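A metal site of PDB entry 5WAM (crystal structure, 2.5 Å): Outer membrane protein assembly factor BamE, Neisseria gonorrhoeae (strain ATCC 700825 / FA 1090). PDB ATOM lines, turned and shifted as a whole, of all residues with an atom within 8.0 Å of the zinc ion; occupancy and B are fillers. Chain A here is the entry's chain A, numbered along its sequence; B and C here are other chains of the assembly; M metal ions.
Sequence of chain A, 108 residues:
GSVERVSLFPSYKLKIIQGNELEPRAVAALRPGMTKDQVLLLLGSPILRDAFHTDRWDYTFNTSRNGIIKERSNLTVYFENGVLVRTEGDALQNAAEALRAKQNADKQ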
ATOM      1  N   ARG A  49     -15.272 -17.483  35.432  1.00  0.00           N
ATOM      2  CA  ARG A  49     -16.563 -18.144  35.280  1.00  0.00           C
ATOM      3  C   ARG A  49     -16.869 -18.392  33.808  1.00  0.00           C
ATOM      4  O   ARG A  49     -17.227 -19.516  33.421  1.00  0.00           O
ATOM      5  CB  ARG A  49     -17.671 -17.314  35.932  1.00  0.00           C
ATOM      6  CG  ARG A  49     -18.995 -18.034  36.066  1.00  0.00           C
ATOM      7  CD  ARG A  49     -19.785 -17.500  37.237  1.00  0.00           C
ATOM      8  NE  ARG A  49     -21.127 -18.091  37.329  1.00  0.00           N
ATOM      9  CZ  ARG A  49     -21.405 -19.249  37.924  1.00  0.00           C
ATOM     10  NH1 ARG A  49     -20.446 -19.971  38.489  1.00  0.00           N
ATOM     11  NH2 ARG A  49     -22.664 -19.684  37.950  1.00  0.00           N
ATOM     12  N   ASP A  50     -16.721 -17.367  32.973  1.00  0.00           N
ATOM     13  CA  ASP A  50     -17.038 -17.447  31.551  1.00  0.00           C
ATOM     14  C   ASP A  50     -15.878 -16.846  30.752  1.00  0.00           C
ATOM     15  O   ASP A  50     -15.868 -15.643  30.456  1.00  0.00           O
ATOM     16  CB  ASP A  50     -18.358 -16.734  31.257  1.00  0.00           C
ATOM     17  CG  ASP A  50     -18.824 -16.938  29.824  1.00  0.00           C
ATOM     18  OD1 ASP A  50     -18.080 -17.550  29.027  1.00  0.00           O
ATOM     19  OD2 ASP A  50     -19.946 -16.495  29.501  1.00  0.00           O
ATOM     20  N   ALA A  51     -14.909 -17.691  30.403  1.00  0.00           N
ATOM     21  CA  ALA A  51     -13.767 -17.220  29.616  1.00  0.00           C
ATOM     22  C   ALA A  51     -14.150 -16.924  28.181  1.00  0.00           C
ATOM     23  O   ALA A  51     -13.574 -16.031  27.558  1.00  0.00           O
ATOM     24  CB  ALA A  51     -12.643 -18.252  29.663  1.00  0.00           C
ATOM     25  N   PHE A  52     -15.115 -17.676  27.626  1.00  0.00           N
ATOM     26  CA  PHE A  52     -15.484 -17.498  26.225  1.00  0.00           C
ATOM     27  C   PHE A  52     -15.904 -16.070  25.926  1.00  0.00           C
ATOM     28  O   PHE A  52     -15.722 -15.589  24.796  1.00  0.00           O
ATOM     29  CB  PHE A  52     -16.606 -18.464  25.851  1.00  0.00           C
ATOM     30  CG  PHE A  52     -16.216 -19.916  25.917  1.00  0.00           C
ATOM     31  CD1 PHE A  52     -15.011 -20.351  25.379  1.00  0.00           C
ATOM     32  CD2 PHE A  52     -17.056 -20.837  26.508  1.00  0.00           C
ATOM     33  CE1 PHE A  52     -14.660 -21.682  25.439  1.00  0.00           C
ATOM     34  CE2 PHE A  52     -16.702 -22.181  26.575  1.00  0.00           C
ATOM     35  CZ  PHE A  52     -15.504 -22.595  26.032  1.00  0.00           C
ATOM     36  N   HIS A  53     -16.477 -15.367  26.901  1.00  0.00           N
ATOM     37  CA  HIS A  53     -17.015 -14.038  26.693  1.00  0.00           C
ATOM     38  C   HIS A  53     -16.376 -13.013  27.623  1.00  0.00           C
ATOM     39  O   HIS A  53     -17.009 -12.040  28.034  1.00  0.00           O
ATOM     40  CB  HIS A  53     -18.533 -14.062  26.843  1.00  0.00           C
ATOM     41  CG  HIS A  53     -19.206 -14.946  25.840  1.00  0.00           C
ATOM     42  ND1 HIS A  53     -19.715 -16.189  26.161  1.00  0.00           N
ATOM     43  CD2 HIS A  53     -19.420 -14.785  24.508  1.00  0.00           C
ATOM     44  CE1 HIS A  53     -20.226 -16.743  25.076  1.00  0.00           C
ATOM     45  NE2 HIS A  53     -20.054 -15.914  24.064  1.00  0.00           N
ATOM     46  N   THR A  54     -15.104 -13.226  27.954  1.00  0.00           N
ATOM     47  CA  THR A  54     -14.275 -12.243  28.634  1.00  0.00           C
ATOM     48  C   THR A  54     -13.039 -12.006  27.778  1.00  0.00           C
ATOM     49  O   THR A  54     -12.405 -12.965  27.318  1.00  0.00           O
ATOM     50  CB  THR A  54     -13.864 -12.722  30.027  1.00  0.00           C
ATOM     51  OG1 THR A  54     -15.034 -13.155  30.747  1.00  0.00           O
ATOM     52  CG2 THR A  54     -13.188 -11.602  30.804  1.00  0.00           C
ATOM     53  N   THR B  63     -24.763 -24.166  23.425  1.00  0.00           N
ATOM     54  CA  THR B  63     -23.889 -23.539  22.436  1.00  0.00           C
ATOM     55  C   THR B  63     -22.847 -24.569  22.011  1.00  0.00           C
ATOM     56  O   THR B  63     -22.104 -25.087  22.859  1.00  0.00           O
ATOM     57  CB  THR B  63     -23.213 -22.292  23.000  1.00  0.00           C
ATOM     58  OG1 THR B  63     -24.204 -21.290  23.284  1.00  0.00           O
ATOM     59  CG2 THR B  63     -22.194 -21.718  22.020  1.00  0.00           C
ATOM     60  N   ARG B  65     -19.766 -25.920  19.149  1.00  0.00           N
ATOM     61  CA  ARG B  65     -18.746 -25.571  18.183  1.00  0.00           C
ATOM     62  C   ARG B  65     -17.969 -26.823  17.837  1.00  0.00           C
ATOM     63  O   ARG B  65     -17.484 -27.524  18.727  1.00  0.00           O
ATOM     64  CB  ARG B  65     -17.792 -24.496  18.727  1.00  0.00           C
ATOM     65  CG  ARG B  65     -18.457 -23.162  18.985  1.00  0.00           C
ATOM     66  CD  ARG B  65     -17.415 -22.059  19.166  1.00  0.00           C
ATOM     67  NE  ARG B  65     -16.619 -22.236  20.372  1.00  0.00           N
ATOM     68  CZ  ARG B  65     -17.009 -21.897  21.594  1.00  0.00           C
ATOM     69  NH1 ARG B  65     -16.209 -22.096  22.629  1.00  0.00           N
ATOM     70  NH2 ARG B  65     -18.210 -21.347  21.796  1.00  0.00           N
ATOM     71  N   LYS B  70     -20.155 -26.549  24.207  1.00  0.00           N
ATOM     72  CA  LYS B  70     -19.131 -25.777  24.890  1.00  0.00           C
ATOM     73  C   LYS B  70     -19.660 -24.960  26.048  1.00  0.00           C
ATOM     74  O   LYS B  70     -18.899 -24.662  26.978  1.00  0.00           O
ATOM     75  CB  LYS B  70     -18.438 -24.837  23.895  1.00  0.00           C
ATOM     76  CG  LYS B  70     -17.854 -25.514  22.671  1.00  0.00           C
ATOM     77  CD  LYS B  70     -16.705 -26.461  23.017  1.00  0.00           C
ATOM     78  CE  LYS B  70     -15.469 -25.710  23.464  1.00  0.00           C
ATOM     79  NZ  LYS B  70     -14.301 -26.630  23.661  1.00  0.00           N
ATOM     80  N   GLU B  71     -20.940 -24.589  26.024  1.00  0.00           N
ATOM     81  CA  GLU B  71     -21.441 -23.624  26.992  1.00  0.00           C
ATOM     82  C   GLU B  71     -22.957 -23.703  27.045  1.00  0.00           C
ATOM     83  O   GLU B  71     -23.624 -23.904  26.029  1.00  0.00           O
ATOM     84  CB  GLU B  71     -21.002 -22.208  26.625  1.00  0.00           C
ATOM     85  CG  GLU B  71     -21.409 -21.145  27.628  1.00  0.00           C
ATOM     86  CD  GLU B  71     -20.854 -19.778  27.286  1.00  0.00           C
ATOM     87  OE1 GLU B  71     -20.403 -19.579  26.137  1.00  0.00           O
ATOM     88  OE2 GLU B  71     -20.862 -18.903  28.180  1.00  0.00           O
ATOM     89  N   ARG B  72     -23.503 -23.550  28.254  1.00  0.00           N
ATOM     90  CA  ARG B  72     -24.927 -23.342  28.466  1.00  0.00           C
ATOM     91  C   ARG B  72     -25.168 -21.852  28.641  1.00  0.00           C
ATOM     92  O   ARG B  72     -24.666 -21.244  29.592  1.00  0.00           O
ATOM     93  CB  ARG B  72     -25.426 -24.120  29.682  1.00  0.00           C
ATOM     94  CG  ARG B  72     -26.016 -25.481  29.365  1.00  0.00           C
ATOM     95  CD  ARG B  72     -24.998 -26.426  28.749  1.00  0.00           C
ATOM     96  NE  ARG B  72     -25.586 -27.746  28.502  1.00  0.00           N
ATOM     97  CZ  ARG B  72     -25.621 -28.737  29.394  1.00  0.00           C
ATOM     98  NH1 ARG B  72     -25.116 -28.573  30.614  1.00  0.00           N
ATOM     99  NH2 ARG B  72     -26.181 -29.892  29.063  1.00  0.00           N
ATOM    100  N   SER B  73     -25.930 -21.256  27.720  1.00  0.00           N
ATOM    101  CA  SER B  73     -26.108 -19.820  27.659  1.00  0.00           C
ATOM    102  C   SER B  73     -27.506 -19.471  28.136  1.00  0.00           C
ATOM    103  O   SER B  73     -28.503 -19.959  27.575  1.00  0.00           O
ATOM    104  CB  SER B  73     -25.871 -19.304  26.248  1.00  0.00           C
ATOM    105  OG  SER B  73     -25.554 -17.925  26.255  1.00  0.00           O
ATOM    106  N   ASN B  74     -27.595 -18.629  29.164  1.00  0.00           N
ATOM    107  CA  ASN B  74     -28.867 -18.299  29.790  1.00  0.00           C
ATOM    108  C   ASN B  74     -29.405 -16.968  29.268  1.00  0.00           C
ATOM    109  O   ASN B  74     -28.645 -16.089  28.851  1.00  0.00           O
ATOM    110  CB  ASN B  74     -28.715 -18.220  31.319  1.00  0.00           C
ATOM    111  CG  ASN B  74     -27.872 -17.034  31.752  1.00  0.00           C
ATOM    112  OD1 ASN B  74     -26.738 -16.873  31.326  1.00  0.00           O
ATOM    113  ND2 ASN B  74     -28.441 -16.195  32.616  1.00  0.00           N
ATOM    114  N   GLY B  89     -28.386 -11.737  30.345  1.00  0.00           N
ATOM    115  CA  GLY B  89     -27.886 -13.096  30.284  1.00  0.00           C
ATOM    116  C   GLY B  89     -26.773 -13.251  29.256  1.00  0.00           C
ATOM    117  O   GLY B  89     -26.539 -12.388  28.410  1.00  0.00           O
ATOM    118  N   ASP B  90     -26.093 -14.394  29.356  1.00  0.00           N
ATOM    119  CA  ASP B  90     -24.974 -14.677  28.465  1.00  0.00           C
ATOM    120  C   ASP B  90     -25.424 -14.796  27.013  1.00  0.00           C
ATOM    121  O   ASP B  90     -24.651 -14.475  26.094  1.00  0.00           O
ATOM    122  CB  ASP B  90     -24.278 -15.960  28.907  1.00  0.00           C
ATOM    123  CG  ASP B  90     -23.011 -16.229  28.129  1.00  0.00           C
ATOM    124  OD1 ASP B  90     -22.053 -15.433  28.243  1.00  0.00           O
ATOM    125  OD2 ASP B  90     -22.964 -17.256  27.404  1.00  0.00           O
ATOM    126  N   ALA B  91     -26.667 -15.235  26.779  1.00  0.00           N
ATOM    127  CA  ALA B  91     -27.112 -15.493  25.417  1.00  0.00           C
ATOM    128  C   ALA B  91     -27.070 -14.247  24.546  1.00  0.00           C
ATOM    129  O   ALA B  91     -26.880 -14.344  23.329  1.00  0.00           O
ATOM    130  CB  ALA B  91     -28.528 -16.071  25.444  1.00  0.00           C
ATOM    131  N   GLN B  93     -24.812 -11.654  24.502  1.00  0.00           N
ATOM    132  CA  GLN B  93     -23.469 -11.566  23.938  1.00  0.00           C
ATOM    133  C   GLN B  93     -23.161 -12.792  23.083  1.00  0.00           C
ATOM    134  O   GLN B  93     -22.486 -12.681  22.055  1.00  0.00           O
ATOM    135  CB  GLN B  93     -22.438 -11.420  25.062  1.00  0.00           C
ATOM    136  CG  GLN B  93     -21.013 -11.239  24.573  1.00  0.00           C
ATOM    137  CD  GLN B  93     -20.032 -11.020  25.714  1.00  0.00           C
ATOM    138  OE1 GLN B  93     -20.423 -11.028  26.882  1.00  0.00           O
ATOM    139  NE2 GLN B  93     -18.759 -10.833  25.380  1.00  0.00           N
ATOM    140  N   ASN B  94     -23.641 -13.962  23.491  1.00  0.00           N
ATOM    141  CA  ASN B  94     -23.368 -15.179  22.752  1.00  0.00           C
ATOM    142  C   ASN B  94     -23.926 -15.110  21.337  1.00  0.00           C
ATOM    143  O   ASN B  94     -23.292 -15.578  20.387  1.00  0.00           O
ATOM    144  CB  ASN B  94     -23.938 -16.385  23.509  1.00  0.00           C
ATOM    145  CG  ASN B  94     -23.268 -17.686  23.134  1.00  0.00           C
ATOM    146  OD1 ASN B  94     -23.025 -17.964  21.958  1.00  0.00           O
ATOM    147  ND2 ASN B  94     -22.932 -18.486  24.141  1.00  0.00           N
ATOM    148  N   GLU B  97     -21.950 -12.024  19.192  1.00  0.00           N
ATOM    149  CA  GLU B  97     -20.652 -12.432  18.650  1.00  0.00           C
ATOM    150  C   GLU B  97     -20.776 -13.603  17.684  1.00  0.00           C
ATOM    151  O   GLU B  97     -19.896 -13.767  16.833  1.00  0.00           O
ATOM    152  CB  GLU B  97     -19.707 -12.792  19.794  1.00  0.00           C
ATOM    153  CG  GLU B  97     -19.536 -11.670  20.817  1.00  0.00           C
ATOM    154  CD  GLU B  97     -18.529 -12.017  21.903  1.00  0.00           C
ATOM    155  OE1 GLU B  97     -17.859 -13.061  21.788  1.00  0.00           O
ATOM    156  OE2 GLU B  97     -18.408 -11.231  22.865  1.00  0.00           O
ATOM    157  N   ARG C  49     -27.191 -23.246  33.164  1.00  0.00           N
ATOM    158  CA  ARG C  49     -25.891 -22.603  33.312  1.00  0.00           C
ATOM    159  C   ARG C  49     -25.209 -23.059  34.596  1.00  0.00           C
ATOM    160  O   ARG C  49     -24.035 -23.462  34.574  1.00  0.00           O
ATOM    161  CB  ARG C  49     -26.040 -21.080  33.289  1.00  0.00           C
ATOM    162  CG  ARG C  49     -24.734 -20.326  33.165  1.00  0.00           C
ATOM    163  CD  ARG C  49     -24.944 -18.988  32.494  1.00  0.00           C
ATOM    164  NE  ARG C  49     -23.721 -18.175  32.462  1.00  0.00           N
ATOM    165  CZ  ARG C  49     -22.774 -18.270  31.531  1.00  0.00           C
ATOM    166  NH1 ARG C  49     -22.879 -19.144  30.539  1.00  0.00           N
ATOM    167  NH2 ARG C  49     -21.707 -17.474  31.602  1.00  0.00           N
HETATM  168 ZN    ZN M   1     -20.496 -17.114  27.753  1.00  0.00          ZN
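The guanidinium group (NH1) of Arg 49 of chain C sits close to the side-chain carboxylate (OE2) of Glu 71 of chain B.
The side-chain carboxylate (OE1) of Glu 71 of chain B is in hydrogen-bond range of the side-chain amide nitrogen (ND2) of Asn 94 of chain B (3.4 Å).
The side-chain carboxylate (OD2) of Asp 50 sits close to the guanidinium group (NH2) of Arg 49 of chain C, 2.9 Å away.
OD1 of Asp 50 lies within hydrogen-bond range of N of Phe 52, at 3.3 Å.
O of Asp 50 sits at hydrogen-bond distance from OG1 of Thr 54, at 2.6 Å.
The side-chain carboxylate (OD2) of Asp 90 of chain B sits close to the guanidinium group (NH1) of Arg 49 of chain C (3.7 Å).
The side-chain carboxylate of Asp 90 of chain B sits close to the side-chain hydroxyl of Ser 73 of chain B (2.9 Å).
The backbone NH of Asp 90 of chain B sits at hydrogen-bond distance from the backbone carbonyl oxygen of Asn 74 of chain B, at 3.1 Å.
Of the 20 residues printed, 4 come within 4 Å of the zinc ion.
The zinc ion is bound by the side-chain carboxylate (OE2) of Glu 71 of chain B (1.9 Å), the side-chain carboxylate (OD2) of Asp 50 (1.9 Å), a ring nitrogen (ND1) of His 53 (2.0 Å), the side-chain carboxylate (OD1) of Asp 90 of chain B (2.3 Å) and the side-chain carboxylate (OD2) of Asp 90 of chain B (2.5 Å).
Slightly farther from the zinc ion lies OD1 of Asp 50 (2.8 Å).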
